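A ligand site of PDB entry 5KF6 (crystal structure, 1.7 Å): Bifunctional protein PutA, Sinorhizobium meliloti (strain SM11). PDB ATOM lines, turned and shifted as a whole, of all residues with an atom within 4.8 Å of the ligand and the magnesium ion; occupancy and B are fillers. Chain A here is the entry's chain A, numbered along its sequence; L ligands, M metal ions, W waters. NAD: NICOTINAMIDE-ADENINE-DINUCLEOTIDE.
OG of Ser 785 lies close to N of Val 788 (3.3 Å).
The side-chain carboxylate of Glu 942 sits at hydrogen-bond distance from the backbone NH of Gly 815 (3.0 Å).
The backbone NH (N) of Thr 813 lies within hydrogen-bond range of the backbone carbonyl oxygen (O) of Ser 1018, 3.0 Å away.
The backbone NH (N) of Thr 783 sits at hydrogen-bond distance from the backbone carbonyl oxygen (O) of Ile 705.
The side-chain amino group of Lys 732 is in hydrogen-bond range of the backbone carbonyl oxygen of Gly 763, 2.7 Å away.
The side-chain hydroxyl (OG) of Ser 1018 is in hydrogen-bond range of the backbone carbonyl oxygen (O) of Gly 814 (2.6 Å).
The side-chain hydroxyl (OG) of Ser 1018 lies within hydrogen-bond range of the backbone NH (N) of Leu 972 (3.4 Å).
The backbone NH (N) of Ser 706 is in hydrogen-bond range of the backbone carbonyl oxygen (O) of Lys 732, 3.4 Å away.
No residue comes within 4 Å of the magnesium ion.
Water W6 bridges an oxygen (O1N) of the ligand (2.7 Å) and the side-chain carboxylate (OE1) of Glu 736 (3.1 Å).
Water W3 lies within hydrogen-bond range of the side-chain carboxylate of Glu 735 (2.7 Å) and an oxygen (O5B) of the ligand (3.4 Å).
Water W4 lies within hydrogen-bond range of an oxygen (O2N) of the ligand (2.7 Å) and the side-chain carboxylate of Glu 736 (2.7 Å).
Water W2 lies within hydrogen-bond range of O of Ser 1018, OE1 of Glu 812 and N7N of the ligand.
Water W7 bridges the side-chain carboxylate of Glu 942 and an oxygen (O3D) of the ligand.
An oxygen (O2N) of the ligand lies within hydrogen-bond range of the backbone NH of Trp 708, at 3.0 Å.
OG of Ser 785 lies within hydrogen-bond range of O1A of the ligand.
NZ of Lys 732 sits at hydrogen-bond distance from O2B of the ligand, 2.8 Å away.
O of Thr 813 is in hydrogen-bond range of N7N of the ligand, 2.8 Å away.
The backbone carbonyl oxygen (O) of Ser 706 lies within hydrogen-bond range of an oxygen (O3B) of the ligand, at 2.8 Å.
The side-chain sulfur (SG) of Cys 846 sits close to an oxygen (O7N) of the ligand (3.7 Å).
O1A of the ligand is in hydrogen-bond range of N of Ser 785 (2.8 Å).
The side-chain carboxylate (OE2) of Glu 942 is in hydrogen-bond range of an oxygen (O3D) of the ligand (2.6 Å).
An oxygen (O2B) of the ligand lies within hydrogen-bond range of the side-chain carboxylate (OE1) of Glu 735 (2.7 Å).
The magnesium ion is bound by water W1 (2.1 Å), water W6 (2.1 Å), water W3 (2.1 Å), O2A of the ligand (2.1 Å) and water W5 (2.4 Å).
O of Gly 784 lies close to O4D of the ligand (3.5 Å).
Ile 705 touches the ligand.
Pro 707 touches the ligand (CB to O5D, 3.2 Å).
OD1 of Asn 709 touches C6N of the ligand, 3.3 Å away.
Phe 710 touches the ligand.
Ile 714 touches the ligand (CD1 to C4N, 3.3 Å).
Pro 733 touches the ligand (C to O3B, 3.9 Å).
Ala 734 touches the ligand.
C of Asp 764 touches O2B of the ligand (3.7 Å).
N of Gly 765 touches O2B of the ligand, 3.6 Å away.
Gly 768 touches the ligand.
Ala 769 touches the ligand (N to C2A, 3.5 Å).
Phe 782 touches the ligand.
Thr 783 touches the ligand (CG2 to C4N, 3.4 Å).
CG2 of Val 788 touches O1A of the ligand, at 3.4 Å.
Ile 792 touches the ligand (CD1 to C2A, 3.8 Å).
Glu 812 touches the ligand (C to N7N, 3.3 Å).
Gly 814 touches the ligand.
Phe 944 touches the ligand (CE1 to C2D, 3.5 Å).
Phe 1012 touches the ligand (CE2 to O7N, 3.3 Å).
Ser 1018 touches the ligand.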
ATOM      1  N   ILE A 705      10.559   3.353   9.777  1.00  0.00           N
ATOM      2  CA  ILE A 705      11.481   2.747   8.824  1.00  0.00           C
ATOM      3  C   ILE A 705      11.747   1.325   9.289  1.00  0.00           C
ATOM      4  O   ILE A 705      12.079   1.098  10.451  1.00  0.00           O
ATOM      5  CB  ILE A 705      12.784   3.565   8.733  1.00  0.00           C
ATOM      6  CG1 ILE A 705      12.466   4.932   8.106  1.00  0.00           C
ATOM      7  CG2 ILE A 705      13.839   2.795   7.948  1.00  0.00           C
ATOM      8  CD1 ILE A 705      13.599   5.963   8.191  1.00  0.00           C
ATOM      9  N   SER A 706      11.592   0.368   8.379  1.00  0.00           N
ATOM     10  CA  SER A 706      11.544  -1.040   8.766  1.00  0.00           C
ATOM     11  C   SER A 706      12.462  -1.885   7.916  1.00  0.00           C
ATOM     12  O   SER A 706      12.813  -1.524   6.782  1.00  0.00           O
ATOM     13  CB  SER A 706      10.095  -1.579   8.691  1.00  0.00           C
ATOM     14  OG  SER A 706       9.517  -1.335   7.415  1.00  0.00           O
ATOM     15  N   PRO A 707      12.881  -3.043   8.432  1.00  0.00           N
ATOM     16  CA  PRO A 707      13.820  -3.917   7.742  1.00  0.00           C
ATOM     17  C   PRO A 707      13.084  -4.887   6.813  1.00  0.00           C
ATOM     18  O   PRO A 707      11.874  -5.074   6.895  1.00  0.00           O
ATOM     19  CB  PRO A 707      14.484  -4.678   8.892  1.00  0.00           C
ATOM     20  CG  PRO A 707      13.374  -4.830   9.876  1.00  0.00           C
ATOM     21  CD  PRO A 707      12.620  -3.519   9.810  1.00  0.00           C
ATOM     22  N   TRP A 708      13.867  -5.505   5.925  1.00  0.00           N
ATOM     23  CA  TRP A 708      13.270  -6.435   4.968  1.00  0.00           C
ATOM     24  C   TRP A 708      12.921  -7.773   5.627  1.00  0.00           C
ATOM     25  O   TRP A 708      12.005  -8.453   5.155  1.00  0.00           O
ATOM     26  CB  TRP A 708      14.219  -6.666   3.788  1.00  0.00           C
ATOM     27  CG  TRP A 708      15.354  -7.587   4.108  1.00  0.00           C
ATOM     28  CD1 TRP A 708      16.622  -7.224   4.444  1.00  0.00           C
ATOM     29  CD2 TRP A 708      15.319  -9.016   4.140  1.00  0.00           C
ATOM     30  NE1 TRP A 708      17.381  -8.351   4.718  1.00  0.00           N
ATOM     31  CE2 TRP A 708      16.599  -9.460   4.540  1.00  0.00           C
ATOM     32  CE3 TRP A 708      14.320  -9.972   3.882  1.00  0.00           C
ATOM     33  CZ2 TRP A 708      16.912 -10.809   4.673  1.00  0.00           C
ATOM     34  CZ3 TRP A 708      14.637 -11.315   4.021  1.00  0.00           C
ATOM     35  CH2 TRP A 708      15.925 -11.713   4.417  1.00  0.00           C
ATOM     36  N   ASN A 709      13.608  -8.159   6.698  1.00  0.00           N
ATOM     37  CA  ASN A 709      13.600  -9.571   7.092  1.00  0.00           C
ATOM     38  C   ASN A 709      12.376  -9.984   7.881  1.00  0.00           C
ATOM     39  O   ASN A 709      12.074 -11.181   7.929  1.00  0.00           O
ATOM     40  CB  ASN A 709      14.860  -9.911   7.898  1.00  0.00           C
ATOM     41  CG  ASN A 709      14.842  -9.305   9.274  1.00  0.00           C
ATOM     42  OD1 ASN A 709      14.817  -8.094   9.413  1.00  0.00           O
ATOM     43  ND2 ASN A 709      14.856 -10.151  10.306  1.00  0.00           N
ATOM     44  N   PHE A 710      11.687  -9.041   8.513  1.00  0.00           N
ATOM     45  CA  PHE A 710      10.382  -9.276   9.129  1.00  0.00           C
ATOM     46  C   PHE A 710       9.430  -8.292   8.468  1.00  0.00           C
ATOM     47  O   PHE A 710       9.024  -7.282   9.069  1.00  0.00           O
ATOM     48  CB  PHE A 710      10.409  -9.096  10.653  1.00  0.00           C
ATOM     49  CG  PHE A 710      11.317 -10.075  11.388  1.00  0.00           C
ATOM     50  CD1 PHE A 710      11.348 -11.413  11.055  1.00  0.00           C
ATOM     51  CD2 PHE A 710      12.124  -9.631  12.437  1.00  0.00           C
ATOM     52  CE1 PHE A 710      12.161 -12.307  11.723  1.00  0.00           C
ATOM     53  CE2 PHE A 710      12.944 -10.519  13.141  1.00  0.00           C
ATOM     54  CZ  PHE A 710      12.968 -11.864  12.772  1.00  0.00           C
ATOM     55  N   ILE A 714       7.438  -6.512  11.899  1.00  0.00           N
ATOM     56  CA  ILE A 714       8.049  -5.299  12.460  1.00  0.00           C
ATOM     57  C   ILE A 714       7.438  -4.069  11.815  1.00  0.00           C
ATOM     58  O   ILE A 714       7.199  -3.063  12.493  1.00  0.00           O
ATOM     59  CB  ILE A 714       9.584  -5.345  12.303  1.00  0.00           C
ATOM     60  CG1 ILE A 714      10.110  -6.418  13.248  1.00  0.00           C
ATOM     61  CG2 ILE A 714      10.228  -3.956  12.613  1.00  0.00           C
ATOM     62  CD1 ILE A 714      11.578  -6.346  13.530  1.00  0.00           C
ATOM     63  N   LYS A 732       7.837   3.746   5.676  1.00  0.00           N
ATOM     64  CA  LYS A 732       8.886   3.549   4.678  1.00  0.00           C
ATOM     65  C   LYS A 732       9.380   2.112   4.787  1.00  0.00           C
ATOM     66  O   LYS A 732      10.329   1.839   5.537  1.00  0.00           O
ATOM     67  CB  LYS A 732      10.034   4.540   4.873  1.00  0.00           C
ATOM     68  CG  LYS A 732      10.698   5.050   3.572  1.00  0.00           C
ATOM     69  CD  LYS A 732      11.290   3.921   2.719  1.00  0.00           C
ATOM     70  CE  LYS A 732      12.489   3.266   3.426  1.00  0.00           C
ATOM     71  NZ  LYS A 732      12.996   2.112   2.627  1.00  0.00           N
ATOM     72  N   PRO A 733       8.800   1.174   4.049  1.00  0.00           N
ATOM     73  CA  PRO A 733       9.278  -0.215   4.105  1.00  0.00           C
ATOM     74  C   PRO A 733      10.625  -0.361   3.416  1.00  0.00           C
ATOM     75  O   PRO A 733      11.028   0.436   2.568  1.00  0.00           O
ATOM     76  CB  PRO A 733       8.192  -0.998   3.364  1.00  0.00           C
ATOM     77  CG  PRO A 733       7.619   0.005   2.380  1.00  0.00           C
ATOM     78  CD  PRO A 733       7.725   1.360   3.046  1.00  0.00           C
ATOM     79  N   ALA A 734      11.309  -1.442   3.792  1.00  0.00           N
ATOM     80  CA  ALA A 734      12.530  -1.833   3.110  1.00  0.00           C
ATOM     81  C   ALA A 734      12.310  -1.935   1.610  1.00  0.00           C
ATOM     82  O   ALA A 734      11.253  -2.400   1.148  1.00  0.00           O
ATOM     83  CB  ALA A 734      13.018  -3.181   3.659  1.00  0.00           C
ATOM     84  N   GLU A 735      13.309  -1.503   0.837  1.00  0.00           N
ATOM     85  CA  GLU A 735      13.203  -1.571  -0.619  1.00  0.00           C
ATOM     86  C   GLU A 735      13.040  -3.004  -1.115  1.00  0.00           C
ATOM     87  O   GLU A 735      12.451  -3.234  -2.170  1.00  0.00           O
ATOM     88  CB  GLU A 735      14.415  -0.916  -1.261  1.00  0.00           C
ATOM     89  CG  GLU A 735      15.755  -1.505  -0.834  1.00  0.00           C
ATOM     90  CD  GLU A 735      16.387  -0.739   0.329  1.00  0.00           C
ATOM     91  OE1 GLU A 735      15.644  -0.132   1.137  1.00  0.00           O
ATOM     92  OE2 GLU A 735      17.631  -0.749   0.440  1.00  0.00           O
ATOM     93  N   GLU A 736      13.524  -3.989  -0.341  1.00  0.00           N
ATOM     94  CA  GLU A 736      13.454  -5.364  -0.789  1.00  0.00           C
ATOM     95  C   GLU A 736      12.037  -5.918  -0.759  1.00  0.00           C
ATOM     96  O   GLU A 736      11.699  -6.779  -1.588  1.00  0.00           O
ATOM     97  CB  GLU A 736      14.376  -6.258   0.058  1.00  0.00           C
ATOM     98  CG  GLU A 736      15.854  -5.981  -0.102  1.00  0.00           C
ATOM     99  CD  GLU A 736      16.380  -4.973   0.891  1.00  0.00           C
ATOM    100  OE1 GLU A 736      17.621  -4.856   1.017  1.00  0.00           O
ATOM    101  OE2 GLU A 736      15.554  -4.314   1.561  1.00  0.00           O
ATOM    102  N   GLY A 763      10.451   2.623  -1.386  1.00  0.00           N
ATOM    103  CA  GLY A 763      11.721   3.115  -1.871  1.00  0.00           C
ATOM    104  C   GLY A 763      12.907   2.702  -1.018  1.00  0.00           C
ATOM    105  O   GLY A 763      12.762   1.977  -0.028  1.00  0.00           O
ATOM    106  N   ASP A 764      14.089   3.181  -1.379  1.00  0.00           N
ATOM    107  CA  ASP A 764      15.309   2.751  -0.710  1.00  0.00           C
ATOM    108  C   ASP A 764      15.659   3.721   0.431  1.00  0.00           C
ATOM    109  O   ASP A 764      14.816   4.488   0.891  1.00  0.00           O
ATOM    110  CB  ASP A 764      16.442   2.617  -1.736  1.00  0.00           C
ATOM    111  CG  ASP A 764      16.670   3.896  -2.521  1.00  0.00           C
ATOM    112  OD1 ASP A 764      16.550   4.984  -1.931  1.00  0.00           O
ATOM    113  OD2 ASP A 764      16.964   3.820  -3.725  1.00  0.00           O
ATOM    114  N   GLY A 765      16.909   3.696   0.873  1.00  0.00           N
ATOM    115  CA  GLY A 765      17.323   4.542   1.984  1.00  0.00           C
ATOM    116  C   GLY A 765      17.197   6.029   1.720  1.00  0.00           C
ATOM    117  O   GLY A 765      17.091   6.807   2.681  1.00  0.00           O
ATOM    118  N   GLY A 768      13.887   6.965   3.039  1.00  0.00           N
ATOM    119  CA  GLY A 768      13.952   7.037   4.488  1.00  0.00           C
ATOM    120  C   GLY A 768      14.680   8.286   4.959  1.00  0.00           C
ATOM    121  O   GLY A 768      14.256   8.956   5.890  1.00  0.00           O
ATOM    122  N   ALA A 769      15.782   8.626   4.285  1.00  0.00           N
ATOM    123  CA  ALA A 769      16.555   9.784   4.707  1.00  0.00           C
ATOM    124  C   ALA A 769      15.794  11.083   4.451  1.00  0.00           C
ATOM    125  O   ALA A 769      15.865  12.019   5.252  1.00  0.00           O
ATOM    126  CB  ALA A 769      17.906   9.799   3.996  1.00  0.00           C
ATOM    127  N   VAL A 772      13.233  11.375   7.300  1.00  0.00           N
ATOM    128  CA  VAL A 772      13.853  11.746   8.572  1.00  0.00           C
ATOM    129  C   VAL A 772      14.194  13.225   8.592  1.00  0.00           C
ATOM    130  O   VAL A 772      13.998  13.914   9.594  1.00  0.00           O
ATOM    131  CB  VAL A 772      15.095  10.868   8.837  1.00  0.00           C
ATOM    132  CG1 VAL A 772      15.865  11.375  10.055  1.00  0.00           C
ATOM    133  CG2 VAL A 772      14.682   9.437   9.061  1.00  0.00           C
ATOM    134  N   PHE A 782      12.929   3.225  14.050  1.00  0.00           N
ATOM    135  CA  PHE A 782      13.842   2.557  13.135  1.00  0.00           C
ATOM    136  C   PHE A 782      14.141   1.165  13.641  1.00  0.00           C
ATOM    137  O   PHE A 782      14.528   0.983  14.798  1.00  0.00           O
ATOM    138  CB  PHE A 782      15.165   3.325  13.017  1.00  0.00           C
ATOM    139  CG  PHE A 782      16.159   2.610  12.156  1.00  0.00           C
ATOM    140  CD1 PHE A 782      16.075   2.703  10.777  1.00  0.00           C
ATOM    141  CD2 PHE A 782      17.161   1.810  12.721  1.00  0.00           C
ATOM    142  CE1 PHE A 782      16.977   2.047   9.954  1.00  0.00           C
ATOM    143  CE2 PHE A 782      18.062   1.145  11.907  1.00  0.00           C
ATOM    144  CZ  PHE A 782      17.966   1.262  10.512  1.00  0.00           C
ATOM    145  N   THR A 783      14.022   0.189  12.741  1.00  0.00           N
ATOM    146  CA  THR A 783      14.545  -1.149  12.967  1.00  0.00           C
ATOM    147  C   THR A 783      15.363  -1.526  11.742  1.00  0.00           C
ATOM    148  O   THR A 783      14.895  -1.376  10.612  1.00  0.00           O
ATOM    149  CB  THR A 783      13.419  -2.160  13.225  1.00  0.00           C
ATOM    150  OG1 THR A 783      12.643  -1.765  14.369  1.00  0.00           O
ATOM    151  CG2 THR A 783      14.019  -3.503  13.544  1.00  0.00           C
ATOM    152  N   GLY A 784      16.581  -2.004  11.951  1.00  0.00           N
ATOM    153  CA  GLY A 784      17.511  -2.201  10.862  1.00  0.00           C
ATOM    154  C   GLY A 784      18.922  -2.320  11.412  1.00  0.00           C
ATOM    155  O   GLY A 784      19.111  -2.583  12.586  1.00  0.00           O
ATOM    156  N   SER A 785      19.887  -2.115  10.527  1.00  0.00           N
ATOM    157  CA  SER A 785      21.300  -2.277  10.896  1.00  0.00           C
ATOM    158  C   SER A 785      21.776  -1.152  11.804  1.00  0.00           C
ATOM    159  O   SER A 785      21.296  -0.014  11.752  1.00  0.00           O
ATOM    160  CB  SER A 785      22.175  -2.328   9.633  1.00  0.00           C
ATOM    161  OG  SER A 785      22.143  -1.117   8.897  1.00  0.00           O
ATOM    162  N   VAL A 788      23.119   1.936   9.810  1.00  0.00           N
ATOM    163  CA  VAL A 788      22.114   2.868   9.304  1.00  0.00           C
ATOM    164  C   VAL A 788      21.501   3.666  10.447  1.00  0.00           C
ATOM    165  O   VAL A 788      21.300   4.882  10.323  1.00  0.00           O
ATOM    166  CB  VAL A 788      21.052   2.115   8.484  1.00  0.00           C
ATOM    167  CG1 VAL A 788      19.871   3.040   8.208  1.00  0.00           C
ATOM    168  CG2 VAL A 788      21.673   1.674   7.146  1.00  0.00           C
ATOM    169  N   LEU A 791      23.590   6.622  11.158  1.00  0.00           N
ATOM    170  CA  LEU A 791      23.378   7.740  10.230  1.00  0.00           C
ATOM    171  C   LEU A 791      22.120   8.516  10.577  1.00  0.00           C
ATOM    172  O   LEU A 791      22.108   9.751  10.475  1.00  0.00           O
ATOM    173  CB  LEU A 791      23.299   7.221   8.801  1.00  0.00           C
ATOM    174  CG  LEU A 791      24.578   6.625   8.206  1.00  0.00           C
ATOM    175  CD1 LEU A 791      24.243   5.827   6.975  1.00  0.00           C
ATOM    176  CD2 LEU A 791      25.571   7.726   7.904  1.00  0.00           C
ATOM    177  N   ILE A 792      21.040   7.827  10.952  1.00  0.00           N
ATOM    178  CA  ILE A 792      19.828   8.534  11.369  1.00  0.00           C
ATOM    179  C   ILE A 792      20.082   9.344  12.631  1.00  0.00           C
ATOM    180  O   ILE A 792      19.685  10.522  12.734  1.00  0.00           O
ATOM    181  CB  ILE A 792      18.674   7.537  11.553  1.00  0.00           C
ATOM    182  CG1 ILE A 792      18.275   7.000  10.180  1.00  0.00           C
ATOM    183  CG2 ILE A 792      17.487   8.210  12.243  1.00  0.00           C
ATOM    184  CD1 ILE A 792      17.404   5.770  10.239  1.00  0.00           C
ATOM    185  N   GLU A 812      16.190  -0.054  16.892  1.00  0.00           N
ATOM    186  CA  GLU A 812      16.386  -1.444  17.279  1.00  0.00           C
ATOM    187  C   GLU A 812      17.274  -2.110  16.219  1.00  0.00           C
ATOM    188  O   GLU A 812      16.901  -2.157  15.047  1.00  0.00           O
ATOM    189  CB  GLU A 812      15.031  -2.125  17.443  1.00  0.00           C
ATOM    190  CG  GLU A 812      14.184  -1.410  18.502  1.00  0.00           C
ATOM    191  CD  GLU A 812      14.842  -1.426  19.903  1.00  0.00           C
ATOM    192  OE1 GLU A 812      14.748  -2.469  20.574  1.00  0.00           O
ATOM    193  OE2 GLU A 812      15.449  -0.423  20.330  1.00  0.00           O
ATOM    194  N   THR A 813      18.462  -2.565  16.617  1.00  0.00           N
ATOM    195  CA  THR A 813      19.523  -2.806  15.655  1.00  0.00           C
ATOM    196  C   THR A 813      20.049  -4.235  15.781  1.00  0.00           C
ATOM    197  O   THR A 813      19.352  -5.143  16.234  1.00  0.00           O
ATOM    198  CB  THR A 813      20.588  -1.697  15.806  1.00  0.00           C
ATOM    199  OG1 THR A 813      20.898  -1.496  17.186  1.00  0.00           O
ATOM    200  CG2 THR A 813      20.024  -0.392  15.243  1.00  0.00           C
ATOM    201  N   GLY A 814      21.267  -4.469  15.291  1.00  0.00           N
ATOM    202  CA  GLY A 814      21.748  -5.817  15.062  1.00  0.00           C
ATOM    203  C   GLY A 814      22.126  -6.552  16.343  1.00  0.00           C
ATOM    204  O   GLY A 814      22.031  -6.037  17.453  1.00  0.00           O
ATOM    205  N   GLY A 815      22.568  -7.802  16.169  1.00  0.00           N
ATOM    206  CA  GLY A 815      23.041  -8.592  17.279  1.00  0.00           C
ATOM    207  C   GLY A 815      24.281  -9.385  16.897  1.00  0.00           C
ATOM    208  O   GLY A 815      24.668  -9.436  15.728  1.00  0.00           O
ATOM    209  N   CYS A 846      17.217 -11.048  13.341  1.00  0.00           N
ATOM    210  CA  CYS A 846      18.123 -10.280  14.194  1.00  0.00           C
ATOM    211  C   CYS A 846      18.513 -11.090  15.431  1.00  0.00           C
ATOM    212  O   CYS A 846      19.599 -10.883  15.978  1.00  0.00           O
ATOM    213  CB  CYS A 846      17.466  -8.975  14.625  1.00  0.00           C
ATOM    214  SG  CYS A 846      15.799  -9.178  15.308  1.00  0.00           S
ATOM    215  N   GLU A 942      28.109  -8.031  12.929  1.00  0.00           N
ATOM    216  CA  GLU A 942      27.046  -8.973  12.606  1.00  0.00           C
ATOM    217  C   GLU A 942      27.149  -9.434  11.164  1.00  0.00           C
ATOM    218  O   GLU A 942      27.325  -8.628  10.244  1.00  0.00           O
ATOM    219  CB  GLU A 942      25.686  -8.305  12.865  1.00  0.00           C
ATOM    220  CG  GLU A 942      24.464  -9.113  12.424  1.00  0.00           C
ATOM    221  CD  GLU A 942      23.198  -8.281  12.480  1.00  0.00           C
ATOM    222  OE1 GLU A 942      22.271  -8.622  13.253  1.00  0.00           O
ATOM    223  OE2 GLU A 942      23.137  -7.267  11.758  1.00  0.00           O
ATOM    224  N   PHE A 944      24.780 -11.209   8.660  1.00  0.00           N
ATOM    225  CA  PHE A 944      23.343 -11.457   8.632  1.00  0.00           C
ATOM    226  C   PHE A 944      23.022 -12.528   7.590  1.00  0.00           C
ATOM    227  O   PHE A 944      22.525 -12.250   6.494  1.00  0.00           O
ATOM    228  CB  PHE A 944      22.595 -10.153   8.362  1.00  0.00           C
ATOM    229  CG  PHE A 944      21.171 -10.166   8.788  1.00  0.00           C
ATOM    230  CD1 PHE A 944      20.828 -10.169  10.141  1.00  0.00           C
ATOM    231  CD2 PHE A 944      20.149 -10.172   7.846  1.00  0.00           C
ATOM    232  CE1 PHE A 944      19.490 -10.191  10.530  1.00  0.00           C
ATOM    233  CE2 PHE A 944      18.811 -10.194   8.235  1.00  0.00           C
ATOM    234  CZ  PHE A 944      18.494 -10.206   9.579  1.00  0.00           C
ATOM    235  N   LEU A 972      21.607  -8.369  22.239  1.00  0.00           N
ATOM    236  CA  LEU A 972      20.236  -8.641  21.804  1.00  0.00           C
ATOM    237  C   LEU A 972      19.713  -9.940  22.420  1.00  0.00           C
ATOM    238  O   LEU A 972      19.073  -9.908  23.470  1.00  0.00           O
ATOM    239  CB  LEU A 972      20.151  -8.675  20.283  1.00  0.00           C
ATOM    240  CG  LEU A 972      18.736  -8.745  19.689  1.00  0.00           C
ATOM    241  CD1 LEU A 972      17.817  -7.713  20.316  1.00  0.00           C
ATOM    242  CD2 LEU A 972      18.828  -8.514  18.170  1.00  0.00           C
ATOM    243  N   PHE A1012      10.611  -7.756  23.236  1.00  0.00           N
ATOM    244  CA  PHE A1012      11.807  -8.029  22.451  1.00  0.00           C
ATOM    245  C   PHE A1012      12.600  -6.749  22.204  1.00  0.00           C
ATOM    246  O   PHE A1012      12.039  -5.747  21.741  1.00  0.00           O
ATOM    247  CB  PHE A1012      11.459  -8.692  21.105  1.00  0.00           C
ATOM    248  CG  PHE A1012      12.686  -9.141  20.366  1.00  0.00           C
ATOM    249  CD1 PHE A1012      13.310 -10.332  20.705  1.00  0.00           C
ATOM    250  CD2 PHE A1012      13.260  -8.342  19.393  1.00  0.00           C
ATOM    251  CE1 PHE A1012      14.445 -10.738  20.067  1.00  0.00           C
ATOM    252  CE2 PHE A1012      14.415  -8.740  18.733  1.00  0.00           C
ATOM    253  CZ  PHE A1012      15.006  -9.948  19.065  1.00  0.00           C
ATOM    254  N   SER A1018      22.745  -3.017  20.123  1.00  0.00           N
ATOM    255  CA  SER A1018      21.555  -3.711  19.654  1.00  0.00           C
ATOM    256  C   SER A1018      20.268  -2.918  19.830  1.00  0.00           C
ATOM    257  O   SER A1018      19.209  -3.380  19.381  1.00  0.00           O
ATOM    258  CB  SER A1018      21.420  -5.069  20.356  1.00  0.00           C
ATOM    259  OG  SER A1018      22.517  -5.927  20.017  1.00  0.00           O
HETATM  260  PA  NAD L   1      18.980  -1.884   6.860  1.00  0.00           P
HETATM  261  O1A NAD L   1      19.822  -1.096   7.899  1.00  0.00           O
HETATM  262  O2A NAD L   1      19.656  -2.331   5.664  1.00  0.00           O
HETATM  263  O5B NAD L   1      17.792  -1.194   6.285  1.00  0.00           O
HETATM  264  C5B NAD L   1      16.731  -0.861   7.169  1.00  0.00           C
HETATM  265  C4B NAD L   1      15.840   0.301   6.682  1.00  0.00           C
HETATM  266  O4B NAD L   1      16.548   1.519   6.737  1.00  0.00           O
HETATM  267  C3B NAD L   1      15.317   0.100   5.279  1.00  0.00           C
HETATM  268  O3B NAD L   1      13.984   0.450   5.172  1.00  0.00           O
HETATM  269  C2B NAD L   1      16.218   0.978   4.486  1.00  0.00           C
HETATM  270  O2B NAD L   1      15.634   1.406   3.299  1.00  0.00           O
HETATM  271  C1B NAD L   1      16.410   2.087   5.455  1.00  0.00           C
HETATM  272  N9A NAD L   1      17.577   2.908   5.218  1.00  0.00           N
HETATM  273  C8A NAD L   1      18.772   2.567   4.614  1.00  0.00           C
HETATM  274  N7A NAD L   1      19.574   3.635   4.643  1.00  0.00           N
HETATM  275  C5A NAD L   1      18.933   4.707   5.253  1.00  0.00           C
HETATM  276  C6A NAD L   1      19.251   6.009   5.534  1.00  0.00           C
HETATM  277  N6A NAD L   1      20.545   6.531   5.177  1.00  0.00           N
HETATM  278  N1A NAD L   1      18.380   6.805   6.160  1.00  0.00           N
HETATM  279  C2A NAD L   1      17.148   6.364   6.518  1.00  0.00           C
HETATM  280  N3A NAD L   1      16.791   5.090   6.253  1.00  0.00           N
HETATM  281  C4A NAD L   1      17.648   4.255   5.629  1.00  0.00           C
HETATM  282  O3  NAD L   1      18.435  -3.186   7.414  1.00  0.00           O
HETATM  283  PN  NAD L   1      17.780  -4.509   6.774  1.00  0.00           P
HETATM  284  O1N NAD L   1      18.816  -5.237   5.960  1.00  0.00           O
HETATM  285  O2N NAD L   1      16.522  -4.178   6.008  1.00  0.00           O
HETATM  286  O5D NAD L   1      17.451  -5.440   8.025  1.00  0.00           O
HETATM  287  C5D NAD L   1      18.452  -6.212   8.626  1.00  0.00           C
HETATM  288  C4D NAD L   1      18.992  -5.599   9.916  1.00  0.00           C
HETATM  289  O4D NAD L   1      17.927  -5.319  10.778  1.00  0.00           O
HETATM  290  C3D NAD L   1      19.953  -6.489  10.619  1.00  0.00           C
HETATM  291  O3D NAD L   1      21.091  -5.794  11.029  1.00  0.00           O
HETATM  292  C2D NAD L   1      19.167  -6.966  11.783  1.00  0.00           C
HETATM  293  O2D NAD L   1      19.963  -7.396  12.852  1.00  0.00           O
HETATM  294  C1D NAD L   1      18.322  -5.764  12.054  1.00  0.00           C
HETATM  295  N1N NAD L   1      17.140  -6.079  12.791  1.00  0.00           N
HETATM  296  C2N NAD L   1      17.027  -5.724  14.158  1.00  0.00           C
HETATM  297  C3N NAD L   1      15.869  -6.086  14.830  1.00  0.00           C
HETATM  298  C7N NAD L   1      15.647  -5.780  16.277  1.00  0.00           C
HETATM  299  O7N NAD L   1      14.556  -6.054  16.779  1.00  0.00           O
HETATM  300  N7N NAD L   1      16.679  -5.206  17.062  1.00  0.00           N
HETATM  301  C4N NAD L   1      14.824  -6.758  14.138  1.00  0.00           C
HETATM  302  C5N NAD L   1      14.950  -7.136  12.787  1.00  0.00           C
HETATM  303  C6N NAD L   1      16.114  -6.792  12.128  1.00  0.00           C
HETATM  304 MG    MG M   1      20.057  -2.390   3.581  1.00  0.00          MG
HETATM  305  O   HOH W   1      21.941  -3.077   4.038  1.00  0.00           O
HETATM  306  O   HOH W   2      16.744  -4.144  19.945  1.00  0.00           O
HETATM  307  O   HOH W   3      18.389  -1.268   2.989  1.00  0.00           O
HETATM  308  O   HOH W   4      16.453  -2.822   3.678  1.00  0.00           O
HETATM  309  O   HOH W   5      21.165  -0.289   3.838  1.00  0.00           O
HETATM  310  O   HOH W   6      19.304  -4.320   3.504  1.00  0.00           O
HETATM  311  O   HOH W   7      23.677  -4.393  12.719  1.00  0.00           O
HETATM  312  O   HOH W   8      12.219  -5.098  17.732  1.00  0.00           O
HETATM  313  O   HOH W   9      21.460   9.704   6.107  1.00  0.00           O
HETATM  314  O   HOH W  10      19.001   9.410   7.481  1.00  0.00           O
